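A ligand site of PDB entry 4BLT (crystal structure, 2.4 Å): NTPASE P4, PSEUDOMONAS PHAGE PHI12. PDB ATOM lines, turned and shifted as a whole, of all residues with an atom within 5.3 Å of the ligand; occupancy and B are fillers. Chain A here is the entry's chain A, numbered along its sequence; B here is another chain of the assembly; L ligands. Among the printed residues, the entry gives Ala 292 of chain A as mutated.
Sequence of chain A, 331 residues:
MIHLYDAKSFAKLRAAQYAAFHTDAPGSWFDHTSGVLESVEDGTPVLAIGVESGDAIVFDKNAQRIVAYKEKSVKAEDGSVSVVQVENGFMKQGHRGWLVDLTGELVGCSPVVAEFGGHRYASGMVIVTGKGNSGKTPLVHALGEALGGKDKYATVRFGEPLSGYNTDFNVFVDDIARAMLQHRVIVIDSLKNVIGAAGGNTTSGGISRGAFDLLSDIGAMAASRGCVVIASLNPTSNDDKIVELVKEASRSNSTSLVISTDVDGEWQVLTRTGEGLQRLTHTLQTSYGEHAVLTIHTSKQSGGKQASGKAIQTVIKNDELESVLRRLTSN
The side-chain amino group (NZ) of Lys 192 lies within salt-bridge range of the side-chain carboxylate (OE2) of Glu 160, 2.9 Å away.
OD1 of Asn 234 lies within hydrogen-bond range of NZ of Lys 136, at 3.2 Å.
The guanidinium group (NH1) of Arg 279 of chain B sits at hydrogen-bond distance from the backbone carbonyl oxygen (O) of Arg 251 of chain B, 3.3 Å away.
The backbone NH (N) of Ile 316 of chain B lies within hydrogen-bond range of the backbone carbonyl oxygen (O) of Arg 279 of chain B (3.0 Å).
The guanidinium group (NH2) of Arg 272 of chain B is in salt-bridge range of the side-chain carboxylate (OE1) of Glu 160 (2.5 Å).
NH1 of Arg 272 of chain B is in hydrogen-bond range of O of Ser 252 of chain B, 3.4 Å away.
OD1 of Asn 133 lies within hydrogen-bond range of N of Asn 318 of chain B (3.2 Å).
The side-chain amino group of Lys 192 is in salt-bridge range of an oxygen (O2) of the ligand (2.7 Å).
The backbone NH (N) of Lys 136 sits at hydrogen-bond distance from an oxygen (O7) of the ligand, at 2.8 Å.
An oxygen (O2) of the ligand sits at hydrogen-bond distance from the side-chain amide nitrogen (ND2) of Asn 234 (2.8 Å).
O1 of the ligand lies within salt-bridge range of NH2 of Arg 279 of chain B (3.1 Å).
An oxygen (O4) of the ligand is in hydrogen-bond range of the side-chain hydroxyl of Thr 137, at 3.3 Å.
The guanidinium group (NH2) of Arg 272 of chain B is in salt-bridge range of an oxygen (O3) of the ligand (3.3 Å).
The side-chain carboxylate of Glu 160 sits close to an oxygen (O3) of the ligand (3.2 Å).
A nitrogen (N1) of the ligand sits close to the side-chain hydroxyl of Tyr 288.
Merely in contact with the ligand: Gly 135 (3.3 Å), Ala 292 (3.8 Å), Ser 252 of chain B (3.5 Å), Gly 276 of chain B (3.3 Å), Leu 277 of chain B (3.8 Å), Gln 278 of chain B (3.3 Å) and Asn 318 of chain B (3.6 Å).
Hydrophobic or aromatic side chains within 4 Å of the ligand: Tyr 288 and Ala 292.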
ATOM      1  N   ASN A 133      22.683   6.549 -11.278  1.00  0.00           N
ATOM      2  CA  ASN A 133      22.118   7.201 -10.093  1.00  0.00           C
ATOM      3  C   ASN A 133      23.046   7.267  -8.876  1.00  0.00           C
ATOM      4  O   ASN A 133      22.695   7.881  -7.874  1.00  0.00           O
ATOM      5  CB  ASN A 133      20.811   6.526  -9.710  1.00  0.00           C
ATOM      6  CG  ASN A 133      19.796   6.520 -10.854  1.00  0.00           C
ATOM      7  OD1 ASN A 133      19.774   7.433 -11.683  1.00  0.00           O
ATOM      8  ND2 ASN A 133      18.940   5.500 -10.881  1.00  0.00           N
ATOM      9  N   SER A 134      24.218   6.648  -8.973  1.00  0.00           N
ATOM     10  CA  SER A 134      25.172   6.650  -7.865  1.00  0.00           C
ATOM     11  C   SER A 134      25.852   8.010  -7.733  1.00  0.00           C
ATOM     12  O   SER A 134      26.499   8.480  -8.676  1.00  0.00           O
ATOM     13  CB  SER A 134      26.207   5.543  -8.039  1.00  0.00           C
ATOM     14  OG  SER A 134      25.609   4.273  -7.919  1.00  0.00           O
ATOM     15  N   GLY A 135      25.708   8.630  -6.563  1.00  0.00           N
ATOM     16  CA  GLY A 135      26.210   9.984  -6.328  1.00  0.00           C
ATOM     17  C   GLY A 135      27.709  10.093  -6.162  1.00  0.00           C
ATOM     18  O   GLY A 135      28.323   9.320  -5.427  1.00  0.00           O
ATOM     19  N   LYS A 136      28.295  11.084  -6.829  1.00  0.00           N
ATOM     20  CA  LYS A 136      29.739  11.308  -6.797  1.00  0.00           C
ATOM     21  C   LYS A 136      30.179  11.971  -5.491  1.00  0.00           C
ATOM     22  O   LYS A 136      31.152  11.528  -4.878  1.00  0.00           O
ATOM     23  CB  LYS A 136      30.177  12.181  -7.985  1.00  0.00           C
ATOM     24  CG  LYS A 136      30.383  11.425  -9.282  1.00  0.00           C
ATOM     25  CD  LYS A 136      29.091  10.796  -9.765  1.00  0.00           C
ATOM     26  CE  LYS A 136      29.179  10.275 -11.179  1.00  0.00           C
ATOM     27  NZ  LYS A 136      27.820  10.260 -11.785  1.00  0.00           N
ATOM     28  N   THR A 137      29.479  13.031  -5.096  1.00  0.00           N
ATOM     29  CA  THR A 137      29.864  13.809  -3.924  1.00  0.00           C
ATOM     30  C   THR A 137      29.907  12.976  -2.629  1.00  0.00           C
ATOM     31  O   THR A 137      30.887  13.058  -1.888  1.00  0.00           O
ATOM     32  CB  THR A 137      28.960  15.063  -3.762  1.00  0.00           C
ATOM     33  OG1 THR A 137      29.184  15.950  -4.858  1.00  0.00           O
ATOM     34  CG2 THR A 137      29.283  15.806  -2.467  1.00  0.00           C
ATOM     35  N   PRO A 138      28.872  12.166  -2.346  1.00  0.00           N
ATOM     36  CA  PRO A 138      28.941  11.319  -1.152  1.00  0.00           C
ATOM     37  C   PRO A 138      30.072  10.295  -1.199  1.00  0.00           C
ATOM     38  O   PRO A 138      30.638   9.957  -0.165  1.00  0.00           O
ATOM     39  CB  PRO A 138      27.572  10.610  -1.123  1.00  0.00           C
ATOM     40  CG  PRO A 138      26.686  11.455  -1.974  1.00  0.00           C
ATOM     41  CD  PRO A 138      27.569  12.039  -3.035  1.00  0.00           C
ATOM     42  N   GLU A 160      30.223  25.065  -7.656  1.00  0.00           N
ATOM     43  CA  GLU A 160      28.842  24.612  -7.494  1.00  0.00           C
ATOM     44  C   GLU A 160      28.019  25.786  -6.967  1.00  0.00           C
ATOM     45  O   GLU A 160      28.537  26.621  -6.233  1.00  0.00           O
ATOM     46  CB  GLU A 160      28.747  23.439  -6.513  1.00  0.00           C
ATOM     47  CG  GLU A 160      29.518  22.180  -6.911  1.00  0.00           C
ATOM     48  CD  GLU A 160      28.890  21.435  -8.075  1.00  0.00           C
ATOM     49  OE1 GLU A 160      27.654  21.304  -8.131  1.00  0.00           O
ATOM     50  OE2 GLU A 160      29.647  20.981  -8.959  1.00  0.00           O
ATOM     51  N   LYS A 192      34.221  20.161 -12.548  1.00  0.00           N
ATOM     52  CA  LYS A 192      33.372  20.464 -13.709  1.00  0.00           C
ATOM     53  C   LYS A 192      33.731  21.755 -14.417  1.00  0.00           C
ATOM     54  O   LYS A 192      33.775  21.795 -15.641  1.00  0.00           O
ATOM     55  CB  LYS A 192      31.893  20.505 -13.323  1.00  0.00           C
ATOM     56  CG  LYS A 192      31.251  19.126 -13.357  1.00  0.00           C
ATOM     57  CD  LYS A 192      29.734  19.198 -13.360  1.00  0.00           C
ATOM     58  CE  LYS A 192      29.169  19.788 -12.066  1.00  0.00           C
ATOM     59  NZ  LYS A 192      29.370  18.882 -10.905  1.00  0.00           N
ATOM     60  N   ASN A 234      31.319  14.889 -12.752  1.00  0.00           N
ATOM     61  CA  ASN A 234      30.045  14.444 -13.318  1.00  0.00           C
ATOM     62  C   ASN A 234      30.089  14.660 -14.839  1.00  0.00           C
ATOM     63  O   ASN A 234      30.156  15.815 -15.292  1.00  0.00           O
ATOM     64  CB  ASN A 234      28.867  15.235 -12.707  1.00  0.00           C
ATOM     65  CG  ASN A 234      27.593  14.408 -12.606  1.00  0.00           C
ATOM     66  OD1 ASN A 234      27.572  13.251 -12.993  1.00  0.00           O
ATOM     67  ND2 ASN A 234      26.509  15.005 -12.077  1.00  0.00           N
ATOM     68  N   THR A 236      28.378  15.430 -17.562  1.00  0.00           N
ATOM     69  CA  THR A 236      27.038  15.965 -17.792  1.00  0.00           C
ATOM     70  C   THR A 236      26.644  16.030 -19.280  1.00  0.00           C
ATOM     71  O   THR A 236      25.793  15.266 -19.731  1.00  0.00           O
ATOM     72  CB  THR A 236      26.892  17.369 -17.172  1.00  0.00           C
ATOM     73  OG1 THR A 236      27.998  18.185 -17.556  1.00  0.00           O
ATOM     74  CG2 THR A 236      26.835  17.294 -15.644  1.00  0.00           C
ATOM     75  N   TYR A 288      24.002   4.214   2.270  1.00  0.00           N
ATOM     76  CA  TYR A 288      23.800   5.453   3.027  1.00  0.00           C
ATOM     77  C   TYR A 288      23.357   5.155   4.456  1.00  0.00           C
ATOM     78  O   TYR A 288      22.565   4.237   4.687  1.00  0.00           O
ATOM     79  CB  TYR A 288      22.764   6.342   2.331  1.00  0.00           C
ATOM     80  CG  TYR A 288      23.248   6.934   1.008  1.00  0.00           C
ATOM     81  CD1 TYR A 288      23.072   6.249  -0.189  1.00  0.00           C
ATOM     82  CD2 TYR A 288      23.886   8.178   0.964  1.00  0.00           C
ATOM     83  CE1 TYR A 288      23.520   6.788  -1.393  1.00  0.00           C
ATOM     84  CE2 TYR A 288      24.331   8.716  -0.231  1.00  0.00           C
ATOM     85  CZ  TYR A 288      24.148   8.013  -1.411  1.00  0.00           C
ATOM     86  OH  TYR A 288      24.593   8.551  -2.606  1.00  0.00           O
ATOM     87  N   ALA A 292      22.472  11.067   4.970  1.00  0.00           N
ATOM     88  CA  ALA A 292      23.107  10.831   3.661  1.00  0.00           C
ATOM     89  C   ALA A 292      24.628  10.644   3.735  1.00  0.00           C
ATOM     90  O   ALA A 292      25.332  10.973   2.770  1.00  0.00           O
ATOM     91  CB  ALA A 292      22.758  11.968   2.708  1.00  0.00           C
ATOM     92  N   ARG B 251      21.447  22.158 -15.582  1.00  0.00           N
ATOM     93  CA  ARG B 251      21.771  20.998 -14.772  1.00  0.00           C
ATOM     94  C   ARG B 251      22.667  21.343 -13.588  1.00  0.00           C
ATOM     95  O   ARG B 251      22.357  20.992 -12.441  1.00  0.00           O
ATOM     96  CB  ARG B 251      22.467  19.938 -15.633  1.00  0.00           C
ATOM     97  CG  ARG B 251      22.714  18.615 -14.923  1.00  0.00           C
ATOM     98  CD  ARG B 251      23.694  17.737 -15.689  1.00  0.00           C
ATOM     99  NE  ARG B 251      23.102  17.121 -16.873  1.00  0.00           N
ATOM    100  CZ  ARG B 251      23.242  17.556 -18.127  1.00  0.00           C
ATOM    101  NH1 ARG B 251      23.953  18.643 -18.416  1.00  0.00           N
ATOM    102  NH2 ARG B 251      22.661  16.899 -19.118  1.00  0.00           N
ATOM    103  N   SER B 252      23.789  22.011 -13.849  1.00  0.00           N
ATOM    104  CA  SER B 252      24.856  22.111 -12.854  1.00  0.00           C
ATOM    105  C   SER B 252      25.251  23.520 -12.381  1.00  0.00           C
ATOM    106  O   SER B 252      25.917  23.647 -11.364  1.00  0.00           O
ATOM    107  CB  SER B 252      26.103  21.382 -13.363  1.00  0.00           C
ATOM    108  OG  SER B 252      26.496  21.871 -14.630  1.00  0.00           O
ATOM    109  N   ARG B 272      17.827  21.391  -5.702  1.00  0.00           N
ATOM    110  CA  ARG B 272      18.957  20.834  -4.982  1.00  0.00           C
ATOM    111  C   ARG B 272      18.874  21.295  -3.531  1.00  0.00           C
ATOM    112  O   ARG B 272      18.755  22.490  -3.259  1.00  0.00           O
ATOM    113  CB  ARG B 272      20.285  21.280  -5.599  1.00  0.00           C
ATOM    114  CG  ARG B 272      20.500  20.737  -7.000  1.00  0.00           C
ATOM    115  CD  ARG B 272      21.642  21.432  -7.737  1.00  0.00           C
ATOM    116  NE  ARG B 272      22.961  20.999  -7.282  1.00  0.00           N
ATOM    117  CZ  ARG B 272      24.115  21.334  -7.865  1.00  0.00           C
ATOM    118  NH1 ARG B 272      24.131  22.108  -8.951  1.00  0.00           N
ATOM    119  NH2 ARG B 272      25.259  20.883  -7.372  1.00  0.00           N
ATOM    120  N   GLU B 275      24.790  20.102  -0.943  1.00  0.00           N
ATOM    121  CA  GLU B 275      25.970  19.431  -1.469  1.00  0.00           C
ATOM    122  C   GLU B 275      25.851  17.926  -1.276  1.00  0.00           C
ATOM    123  O   GLU B 275      25.782  17.443  -0.154  1.00  0.00           O
ATOM    124  CB  GLU B 275      27.195  20.004  -0.751  1.00  0.00           C
ATOM    125  CG  GLU B 275      28.405  19.117  -0.583  1.00  0.00           C
ATOM    126  CD  GLU B 275      29.432  19.800   0.282  1.00  0.00           C
ATOM    127  OE1 GLU B 275      30.041  20.785  -0.172  1.00  0.00           O
ATOM    128  OE2 GLU B 275      29.598  19.397   1.454  1.00  0.00           O
ATOM    129  N   GLY B 276      25.790  17.196  -2.391  1.00  0.00           N
ATOM    130  CA  GLY B 276      25.679  15.741  -2.382  1.00  0.00           C
ATOM    131  C   GLY B 276      24.410  15.193  -1.758  1.00  0.00           C
ATOM    132  O   GLY B 276      24.412  14.076  -1.240  1.00  0.00           O
ATOM    133  N   LEU B 277      23.335  15.956  -1.817  1.00  0.00           N
ATOM    134  CA  LEU B 277      22.035  15.511  -1.308  1.00  0.00           C
ATOM    135  C   LEU B 277      21.096  15.245  -2.474  1.00  0.00           C
ATOM    136  O   LEU B 277      21.396  15.587  -3.615  1.00  0.00           O
ATOM    137  CB  LEU B 277      21.424  16.527  -0.344  1.00  0.00           C
ATOM    138  CG  LEU B 277      22.263  16.940   0.872  1.00  0.00           C
ATOM    139  CD1 LEU B 277      21.393  17.713   1.860  1.00  0.00           C
ATOM    140  CD2 LEU B 277      22.890  15.737   1.565  1.00  0.00           C
ATOM    141  N   GLN B 278      19.960  14.620  -2.168  1.00  0.00           N
ATOM    142  CA  GLN B 278      18.981  14.299  -3.207  1.00  0.00           C
ATOM    143  C   GLN B 278      18.253  15.543  -3.673  1.00  0.00           C
ATOM    144  O   GLN B 278      18.022  16.476  -2.900  1.00  0.00           O
ATOM    145  CB  GLN B 278      17.979  13.247  -2.711  1.00  0.00           C
ATOM    146  CG  GLN B 278      18.529  11.831  -2.775  1.00  0.00           C
ATOM    147  CD  GLN B 278      17.765  10.846  -1.915  1.00  0.00           C
ATOM    148  OE1 GLN B 278      17.481  11.120  -0.746  1.00  0.00           O
ATOM    149  NE2 GLN B 278      17.412   9.690  -2.484  1.00  0.00           N
ATOM    150  N   ARG B 279      17.889  15.533  -4.955  1.00  0.00           N
ATOM    151  CA  ARG B 279      17.183  16.618  -5.578  1.00  0.00           C
ATOM    152  C   ARG B 279      15.668  16.376  -5.392  1.00  0.00           C
ATOM    153  O   ARG B 279      15.203  15.245  -5.534  1.00  0.00           O
ATOM    154  CB  ARG B 279      17.562  16.656  -7.062  1.00  0.00           C
ATOM    155  CG  ARG B 279      17.617  18.038  -7.701  1.00  0.00           C
ATOM    156  CD  ARG B 279      18.129  17.950  -9.132  1.00  0.00           C
ATOM    157  NE  ARG B 279      19.589  17.813  -9.182  1.00  0.00           N
ATOM    158  CZ  ARG B 279      20.431  18.645  -9.808  1.00  0.00           C
ATOM    159  NH1 ARG B 279      19.999  19.705 -10.481  1.00  0.00           N
ATOM    160  NH2 ARG B 279      21.737  18.386  -9.775  1.00  0.00           N
ATOM    161  N   ILE B 316      14.085  12.701  -6.588  1.00  0.00           N
ATOM    162  CA  ILE B 316      14.262  12.332  -7.987  1.00  0.00           C
ATOM    163  C   ILE B 316      15.677  11.785  -8.207  1.00  0.00           C
ATOM    164  O   ILE B 316      16.658  12.377  -7.742  1.00  0.00           O
ATOM    165  CB  ILE B 316      13.963  13.531  -8.923  1.00  0.00           C
ATOM    166  CG1 ILE B 316      13.790  13.073 -10.363  1.00  0.00           C
ATOM    167  CG2 ILE B 316      15.048  14.600  -8.830  1.00  0.00           C
ATOM    168  CD1 ILE B 316      13.304  14.169 -11.290  1.00  0.00           C
ATOM    169  N   LYS B 317      15.777  10.648  -8.900  1.00  0.00           N
ATOM    170  CA  LYS B 317      17.071  10.055  -9.229  1.00  0.00           C
ATOM    171  C   LYS B 317      17.697  10.746 -10.449  1.00  0.00           C
ATOM    172  O   LYS B 317      17.063  11.590 -11.072  1.00  0.00           O
ATOM    173  CB  LYS B 317      16.920   8.553  -9.492  1.00  0.00           C
ATOM    174  CG  LYS B 317      16.581   7.731  -8.257  1.00  0.00           C
ATOM    175  CD  LYS B 317      17.008   6.283  -8.428  1.00  0.00           C
ATOM    176  CE  LYS B 317      16.703   5.435  -7.195  1.00  0.00           C
ATOM    177  NZ  LYS B 317      15.267   5.050  -7.120  1.00  0.00           N
ATOM    178  N   ASN B 318      18.935  10.368 -10.776  1.00  0.00           N
ATOM    179  CA  ASN B 318      19.660  10.983 -11.904  1.00  0.00           C
ATOM    180  C   ASN B 318      19.069  10.683 -13.287  1.00  0.00           C
ATOM    181  O   ASN B 318      19.056  11.565 -14.151  1.00  0.00           O
ATOM    182  CB  ASN B 318      21.169  10.620 -11.863  1.00  0.00           C
ATOM    183  CG  ASN B 318      22.012  11.669 -11.142  1.00  0.00           C
ATOM    184  OD1 ASN B 318      23.001  11.332 -10.496  1.00  0.00           O
ATOM    185  ND2 ASN B 318      21.632  12.933 -11.263  1.00  0.00           N
HETATM  186  P1  LIG L   1      26.034  18.131 -10.021  1.00  0.00           P
HETATM  187  O1  LIG L   1      24.675  17.474 -10.122  1.00  0.00           O
HETATM  188  O2  LIG L   1      27.131  17.395 -10.763  1.00  0.00           O
HETATM  189  O3  LIG L   1      26.013  19.627 -10.281  1.00  0.00           O
HETATM  190  P2  LIG L   1      26.023  16.734  -7.568  1.00  0.00           P
HETATM  191  O4  LIG L   1      26.376  16.958  -6.148  1.00  0.00           O
HETATM  192  O5  LIG L   1      24.437  16.504  -7.700  1.00  0.00           O
HETATM  193  O6  LIG L   1      26.447  17.997  -8.472  1.00  0.00           O
HETATM  194  P3  LIG L   1      25.930  13.798  -7.883  1.00  0.00           P
HETATM  195  O7  LIG L   1      26.684  12.542  -8.526  1.00  0.00           O
HETATM  196  O8  LIG L   1      24.620  13.961  -8.551  1.00  0.00           O
HETATM  197  C1  LIG L   1      26.936  15.276  -8.148  1.00  0.00           C
HETATM  198  O9  LIG L   1      25.725  13.569  -6.297  1.00  0.00           O
HETATM  199  C2  LIG L   1      24.450  13.686  -5.657  1.00  0.00           C
HETATM  200  C3  LIG L   1      23.585  12.462  -5.926  1.00  0.00           C
HETATM  201  O10 LIG L   1      23.681  11.518  -4.856  1.00  0.00           O
HETATM  202  C4  LIG L   1      22.106  12.804  -6.057  1.00  0.00           C
HETATM  203  O11 LIG L   1      21.725  12.916  -7.434  1.00  0.00           O
HETATM  204  C5  LIG L   1      21.361  11.689  -5.351  1.00  0.00           C
HETATM  205  O12 LIG L   1      20.610  10.903  -6.277  1.00  0.00           O
HETATM  206  C6  LIG L   1      22.425  10.847  -4.659  1.00  0.00           C
HETATM  207  N1  LIG L   1      22.138  10.722  -3.196  1.00  0.00           N
HETATM  208  C7  LIG L   1      22.543  11.584  -2.241  1.00  0.00           C
HETATM  209  N2  LIG L   1      22.096  11.193  -1.012  1.00  0.00           N
HETATM  210  C8  LIG L   1      21.397  10.065  -1.180  1.00  0.00           C
HETATM  211  C9  LIG L   1      20.663   9.124  -0.291  1.00  0.00           C
HETATM  212  N3  LIG L   1      20.600   9.342   1.042  1.00  0.00           N
HETATM  213  N4  LIG L   1      20.062   8.053  -0.867  1.00  0.00           N
HETATM  214  C10 LIG L   1      20.123   7.820  -2.192  1.00  0.00           C
HETATM  215  N5  LIG L   1      20.776   8.632  -3.047  1.00  0.00           N
HETATM  216  C11 LIG L   1      21.426   9.747  -2.618  1.00  0.00           C
